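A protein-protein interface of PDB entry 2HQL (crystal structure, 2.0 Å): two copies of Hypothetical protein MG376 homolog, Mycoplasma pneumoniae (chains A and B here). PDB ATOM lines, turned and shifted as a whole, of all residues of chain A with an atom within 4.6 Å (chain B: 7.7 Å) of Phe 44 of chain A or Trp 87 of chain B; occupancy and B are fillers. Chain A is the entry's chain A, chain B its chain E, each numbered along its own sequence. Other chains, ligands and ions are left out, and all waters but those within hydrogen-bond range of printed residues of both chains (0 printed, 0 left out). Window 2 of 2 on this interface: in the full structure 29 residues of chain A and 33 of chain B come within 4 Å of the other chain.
The guanidinium group of Arg 37 of chain A sits close to the guanidinium group of Arg 77 of chain B (3.2 Å).
The backbone carbonyl oxygen (O) of Thr 78 of chain B is in hydrogen-bond range of the guanidinium group (NH1) of Arg 37 of chain A (2.8 Å).
The backbone NH (N) of Phe 44 of chain A is in hydrogen-bond range of the backbone carbonyl oxygen (O) of Arg 37 of chain A (2.6 Å).
The backbone carbonyl oxygen (O) of Arg 77 of chain B sits at hydrogen-bond distance from the backbone NH (N) of Thr 90 of chain B (2.8 Å).
N of Glu 81 of chain B is in hydrogen-bond range of O of Ile 86 of chain B (2.8 Å).
CH2 of Trp 87 of chain B touches CE2 of Phe 44 of chain A, at 2.9 Å.
Lys 88 of chain A touches Ile 86 of chain B (NZ to CG2, 3.4 Å).
Printed residues of chain B within 4 Å of Arg 37 of chain A: Arg 77 and Thr 78.
Leu 43 of chain A touches none of the printed residues of chain B.
Phe 44 of chain A touches just one residue of chain B: Trp 87.
Of the printed residues of chain A, Thr 78 of chain B touches Arg 37.
Glu 81 of chain B touches none of the printed residues of chain A.
The nearest residue of chain B that does not touch Phe 44 of chain A is Leu 80 of chain B (6.2 Å).
Printed residues of chain B that touch a printed residue of chain A: Arg 77, Thr 78, Ile 86 and Trp 87.
Hydrophobic or aromatic side chains of chain B within 4 Å of the printed part of chain A: Ile 86 and Trp 87.
Hydrophobic or aromatic side chains of chain A that line the printed part of chain B: Phe 44.
1 position is printed for both chains.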
ATOM      1  N   MET A  36     -21.539  -1.367  15.545  1.00  0.00           N
ATOM      2  CA  MET A  36     -20.322  -0.874  14.893  1.00  0.00           C
ATOM      3  C   MET A  36     -20.554   0.381  14.052  1.00  0.00           C
ATOM      4  O   MET A  36     -21.576   0.530  13.383  1.00  0.00           O
ATOM      5  CB  MET A  36     -19.687  -1.978  14.046  1.00  0.00           C
ATOM      6  CG  MET A  36     -19.337  -3.236  14.851  1.00  0.00           C
ATOM      7  SD  MET A  36     -18.521  -2.862  16.437  1.00  0.00           S
ATOM      8  CE  MET A  36     -16.939  -2.207  15.885  1.00  0.00           C
ATOM      9  N   ARG A  37     -19.573   1.276  14.100  1.00  0.00           N
ATOM     10  CA  ARG A  37     -19.612   2.560  13.419  1.00  0.00           C
ATOM     11  C   ARG A  37     -18.260   2.796  12.738  1.00  0.00           C
ATOM     12  O   ARG A  37     -17.236   2.260  13.156  1.00  0.00           O
ATOM     13  CB  ARG A  37     -19.859   3.659  14.471  1.00  0.00           C
ATOM     14  CG  ARG A  37     -19.953   5.104  13.981  1.00  0.00           C
ATOM     15  CD  ARG A  37     -21.263   5.383  13.254  1.00  0.00           C
ATOM     16  NE  ARG A  37     -21.511   6.814  13.122  1.00  0.00           N
ATOM     17  CZ  ARG A  37     -21.834   7.609  14.139  1.00  0.00           C
ATOM     18  NH1 ARG A  37     -21.956   7.106  15.360  1.00  0.00           N
ATOM     19  NH2 ARG A  37     -21.999   8.917  13.949  1.00  0.00           N
ATOM     20  N   ARG A  42     -11.515   4.343  10.128  1.00  0.00           N
ATOM     21  CA  ARG A  42     -11.475   3.784  11.471  1.00  0.00           C
ATOM     22  C   ARG A  42     -12.770   3.077  11.828  1.00  0.00           C
ATOM     23  O   ARG A  42     -13.855   3.596  11.596  1.00  0.00           O
ATOM     24  CB  ARG A  42     -11.191   4.896  12.477  1.00  0.00           C
ATOM     25  CG  ARG A  42      -9.842   5.559  12.264  1.00  0.00           C
ATOM     26  CD  ARG A  42      -8.696   4.566  12.508  1.00  0.00           C
ATOM     27  NE  ARG A  42      -8.916   3.801  13.739  1.00  0.00           N
ATOM     28  CZ  ARG A  42      -7.958   3.383  14.567  1.00  0.00           C
ATOM     29  NH1 ARG A  42      -6.689   3.649  14.318  1.00  0.00           N
ATOM     30  NH2 ARG A  42      -8.276   2.696  15.658  1.00  0.00           N
ATOM     31  N   LEU A  43     -12.652   1.873  12.377  1.00  0.00           N
ATOM     32  CA  LEU A  43     -13.816   1.098  12.782  1.00  0.00           C
ATOM     33  C   LEU A  43     -13.938   1.382  14.272  1.00  0.00           C
ATOM     34  O   LEU A  43     -13.011   1.128  15.049  1.00  0.00           O
ATOM     35  CB  LEU A  43     -13.606  -0.403  12.556  1.00  0.00           C
ATOM     36  CG  LEU A  43     -14.819  -1.265  12.155  1.00  0.00           C
ATOM     37  CD1 LEU A  43     -14.648  -2.632  12.785  1.00  0.00           C
ATOM     38  CD2 LEU A  43     -16.153  -0.655  12.601  1.00  0.00           C
ATOM     39  N   PHE A  44     -15.098   1.902  14.650  1.00  0.00           N
ATOM     40  CA  PHE A  44     -15.362   2.294  16.017  1.00  0.00           C
ATOM     41  C   PHE A  44     -16.645   1.639  16.569  1.00  0.00           C
ATOM     42  O   PHE A  44     -17.047   0.575  16.118  1.00  0.00           O
ATOM     43  CB  PHE A  44     -15.453   3.825  16.054  1.00  0.00           C
ATOM     44  CG  PHE A  44     -15.368   4.393  17.419  1.00  0.00           C
ATOM     45  CD1 PHE A  44     -14.140   4.519  18.060  1.00  0.00           C
ATOM     46  CD2 PHE A  44     -16.527   4.735  18.107  1.00  0.00           C
ATOM     47  CE1 PHE A  44     -14.069   4.978  19.381  1.00  0.00           C
ATOM     48  CE2 PHE A  44     -16.473   5.188  19.418  1.00  0.00           C
ATOM     49  CZ  PHE A  44     -15.241   5.312  20.062  1.00  0.00           C
ATOM     50  N   THR A  45     -17.300   2.287  17.524  1.00  0.00           N
ATOM     51  CA  THR A  45     -18.492   1.718  18.125  1.00  0.00           C
ATOM     52  C   THR A  45     -19.515   2.746  18.620  1.00  0.00           C
ATOM     53  O   THR A  45     -19.165   3.868  18.974  1.00  0.00           O
ATOM     54  CB  THR A  45     -18.069   0.808  19.295  1.00  0.00           C
ATOM     55  OG1 THR A  45     -19.207   0.460  20.084  1.00  0.00           O
ATOM     56  CG2 THR A  45     -17.053   1.525  20.180  1.00  0.00           C
ATOM     57  N   LYS A  88     -30.629  12.485  27.828  1.00  0.00           N
ATOM     58  CA  LYS A  88     -30.092  11.203  27.393  1.00  0.00           C
ATOM     59  C   LYS A  88     -31.159  10.384  26.676  1.00  0.00           C
ATOM     60  O   LYS A  88     -32.341  10.549  26.939  1.00  0.00           O
ATOM     61  CB  LYS A  88     -29.546  10.434  28.610  1.00  0.00           C
ATOM     62  CG  LYS A  88     -28.461  11.177  29.399  1.00  0.00           C
ATOM     63  CD  LYS A  88     -27.131  11.130  28.677  1.00  0.00           C
ATOM     64  CE  LYS A  88     -26.127  12.160  29.217  1.00  0.00           C
ATOM     65  NZ  LYS A  88     -24.885  12.242  28.373  1.00  0.00           N
ATOM     66  N   ARG B  77     -27.533   7.575  15.922  1.00  0.00           N
ATOM     67  CA  ARG B  77     -26.073   7.717  15.969  1.00  0.00           C
ATOM     68  C   ARG B  77     -25.628   8.367  17.287  1.00  0.00           C
ATOM     69  O   ARG B  77     -26.408   9.012  17.968  1.00  0.00           O
ATOM     70  CB  ARG B  77     -25.570   8.621  14.832  1.00  0.00           C
ATOM     71  CG  ARG B  77     -26.325   8.521  13.523  1.00  0.00           C
ATOM     72  CD  ARG B  77     -25.384   8.482  12.330  1.00  0.00           C
ATOM     73  NE  ARG B  77     -24.584   7.252  12.287  1.00  0.00           N
ATOM     74  CZ  ARG B  77     -25.084   6.019  12.343  1.00  0.00           C
ATOM     75  NH1 ARG B  77     -26.386   5.834  12.447  1.00  0.00           N
ATOM     76  NH2 ARG B  77     -24.286   4.966  12.305  1.00  0.00           N
ATOM     77  N   THR B  78     -24.365   8.196  17.650  1.00  0.00           N
ATOM     78  CA  THR B  78     -23.839   8.860  18.841  1.00  0.00           C
ATOM     79  C   THR B  78     -22.504   9.454  18.381  1.00  0.00           C
ATOM     80  O   THR B  78     -21.946   9.038  17.355  1.00  0.00           O
ATOM     81  CB  THR B  78     -23.609   7.871  20.044  1.00  0.00           C
ATOM     82  OG1 THR B  78     -22.394   7.136  19.858  1.00  0.00           O
ATOM     83  CG2 THR B  78     -24.780   6.880  20.159  1.00  0.00           C
ATOM     84  N   TYR B  79     -22.005  10.451  19.090  1.00  0.00           N
ATOM     85  CA  TYR B  79     -20.717  11.023  18.727  1.00  0.00           C
ATOM     86  C   TYR B  79     -20.117  11.622  19.986  1.00  0.00           C
ATOM     87  O   TYR B  79     -20.837  11.926  20.939  1.00  0.00           O
ATOM     88  CB  TYR B  79     -20.880  12.083  17.634  1.00  0.00           C
ATOM     89  CG  TYR B  79     -21.616  13.308  18.084  1.00  0.00           C
ATOM     90  CD1 TYR B  79     -20.930  14.398  18.623  1.00  0.00           C
ATOM     91  CD2 TYR B  79     -23.000  13.380  17.992  1.00  0.00           C
ATOM     92  CE1 TYR B  79     -21.598  15.525  19.053  1.00  0.00           C
ATOM     93  CE2 TYR B  79     -23.684  14.503  18.427  1.00  0.00           C
ATOM     94  CZ  TYR B  79     -22.977  15.570  18.950  1.00  0.00           C
ATOM     95  OH  TYR B  79     -23.645  16.702  19.352  1.00  0.00           O
ATOM     96  N   LEU B  80     -18.801  11.782  19.999  1.00  0.00           N
ATOM     97  CA  LEU B  80     -18.131  12.334  21.161  1.00  0.00           C
ATOM     98  C   LEU B  80     -17.880  13.827  21.018  1.00  0.00           C
ATOM     99  O   LEU B  80     -17.277  14.280  20.049  1.00  0.00           O
ATOM    100  CB  LEU B  80     -16.805  11.619  21.389  1.00  0.00           C
ATOM    101  CG  LEU B  80     -16.440  11.315  22.842  1.00  0.00           C
ATOM    102  CD1 LEU B  80     -15.011  10.825  22.863  1.00  0.00           C
ATOM    103  CD2 LEU B  80     -16.582  12.531  23.726  1.00  0.00           C
ATOM    104  N   GLU B  81     -18.359  14.591  21.989  1.00  0.00           N
ATOM    105  CA  GLU B  81     -18.168  16.025  21.983  1.00  0.00           C
ATOM    106  C   GLU B  81     -16.784  16.272  22.559  1.00  0.00           C
ATOM    107  O   GLU B  81     -16.524  15.960  23.722  1.00  0.00           O
ATOM    108  CB  GLU B  81     -19.216  16.687  22.848  1.00  0.00           C
ATOM    109  CG  GLU B  81     -19.976  17.747  22.106  1.00  0.00           C
ATOM    110  CD  GLU B  81     -21.019  18.391  22.959  1.00  0.00           C
ATOM    111  OE1 GLU B  81     -21.920  19.036  22.393  1.00  0.00           O
ATOM    112  OE2 GLU B  81     -20.929  18.252  24.196  1.00  0.00           O
ATOM    113  N   SER B  84     -15.932  18.869  25.351  1.00  0.00           N
ATOM    114  CA  SER B  84     -17.218  18.758  26.023  1.00  0.00           C
ATOM    115  C   SER B  84     -17.342  17.417  26.729  1.00  0.00           C
ATOM    116  O   SER B  84     -18.257  17.223  27.522  1.00  0.00           O
ATOM    117  CB  SER B  84     -18.346  18.952  25.007  1.00  0.00           C
ATOM    118  OG  SER B  84     -18.153  20.162  24.294  1.00  0.00           O
ATOM    119  N   GLU B  85     -16.414  16.517  26.391  1.00  0.00           N
ATOM    120  CA  GLU B  85     -16.232  15.191  26.983  1.00  0.00           C
ATOM    121  C   GLU B  85     -17.306  14.122  26.817  1.00  0.00           C
ATOM    122  O   GLU B  85     -17.040  12.931  27.001  1.00  0.00           O
ATOM    123  CB  GLU B  85     -15.994  15.363  28.492  1.00  0.00           C
ATOM    124  CG  GLU B  85     -17.306  15.574  29.262  1.00  0.00           C
ATOM    125  CD  GLU B  85     -17.131  16.128  30.687  1.00  0.00           C
ATOM    126  OE1 GLU B  85     -16.365  15.532  31.479  1.00  0.00           O
ATOM    127  OE2 GLU B  85     -17.762  17.165  31.019  1.00  0.00           O
ATOM    128  N   ILE B  86     -18.511  14.542  26.465  1.00  0.00           N
ATOM    129  CA  ILE B  86     -19.658  13.640  26.418  1.00  0.00           C
ATOM    130  C   ILE B  86     -20.049  12.945  25.109  1.00  0.00           C
ATOM    131  O   ILE B  86     -19.936  13.514  24.026  1.00  0.00           O
ATOM    132  CB  ILE B  86     -20.896  14.415  26.970  1.00  0.00           C
ATOM    133  CG1 ILE B  86     -20.660  14.803  28.436  1.00  0.00           C
ATOM    134  CG2 ILE B  86     -22.158  13.572  26.848  1.00  0.00           C
ATOM    135  CD1 ILE B  86     -21.540  15.938  28.943  1.00  0.00           C
ATOM    136  N   TRP B  87     -20.504  11.695  25.226  1.00  0.00           N
ATOM    137  CA  TRP B  87     -20.976  10.903  24.086  1.00  0.00           C
ATOM    138  C   TRP B  87     -22.456  11.249  23.932  1.00  0.00           C
ATOM    139  O   TRP B  87     -23.278  10.790  24.711  1.00  0.00           O
ATOM    140  CB  TRP B  87     -20.859   9.388  24.349  1.00  0.00           C
ATOM    141  CG  TRP B  87     -19.504   8.778  24.060  1.00  0.00           C
ATOM    142  CD1 TRP B  87     -18.507   8.507  24.961  1.00  0.00           C
ATOM    143  CD2 TRP B  87     -18.969   8.460  22.767  1.00  0.00           C
ATOM    144  NE1 TRP B  87     -17.380   8.052  24.305  1.00  0.00           N
ATOM    145  CE2 TRP B  87     -17.637   8.013  22.961  1.00  0.00           C
ATOM    146  CE3 TRP B  87     -19.483   8.513  21.463  1.00  0.00           C
ATOM    147  CZ2 TRP B  87     -16.815   7.625  21.898  1.00  0.00           C
ATOM    148  CZ3 TRP B  87     -18.660   8.125  20.395  1.00  0.00           C
ATOM    149  CH2 TRP B  87     -17.342   7.690  20.622  1.00  0.00           C
ATOM    150  N   LYS B  88     -22.801  12.043  22.923  1.00  0.00           N
ATOM    151  CA  LYS B  88     -24.192  12.456  22.714  1.00  0.00           C
ATOM    152  C   LYS B  88     -24.905  11.615  21.661  1.00  0.00           C
ATOM    153  O   LYS B  88     -24.288  11.184  20.676  1.00  0.00           O
ATOM    154  CB  LYS B  88     -24.238  13.934  22.315  1.00  0.00           C
ATOM    155  CG  LYS B  88     -23.557  14.870  23.302  1.00  0.00           C
ATOM    156  CD  LYS B  88     -23.906  16.342  23.053  1.00  0.00           C
ATOM    157  CE  LYS B  88     -25.317  16.689  23.536  1.00  0.00           C
ATOM    158  NZ  LYS B  88     -25.646  18.148  23.411  1.00  0.00           N
ATOM    159  N   THR B  89     -26.200  11.365  21.874  1.00  0.00           N
ATOM    160  CA  THR B  89     -26.979  10.567  20.930  1.00  0.00           C
ATOM    161  C   THR B  89     -27.857  11.493  20.117  1.00  0.00           C
ATOM    162  O   THR B  89     -28.392  12.471  20.644  1.00  0.00           O
ATOM    163  CB  THR B  89     -27.886   9.513  21.623  1.00  0.00           C
ATOM    164  OG1 THR B  89     -27.091   8.630  22.432  1.00  0.00           O
ATOM    165  CG2 THR B  89     -28.614   8.698  20.582  1.00  0.00           C
ATOM    166  N   THR B  90     -28.001  11.176  18.832  1.00  0.00           N
ATOM    167  CA  THR B  90     -28.792  11.984  17.917  1.00  0.00           C
ATOM    168  C   THR B  90     -29.315  11.134  16.751  1.00  0.00           C
ATOM    169  O   THR B  90     -29.017   9.942  16.655  1.00  0.00           O
ATOM    170  CB  THR B  90     -27.910  13.162  17.389  1.00  0.00           C
ATOM    171  OG1 THR B  90     -28.619  13.897  16.391  1.00  0.00           O
ATOM    172  CG2 THR B  90     -26.592  12.631  16.812  1.00  0.00           C
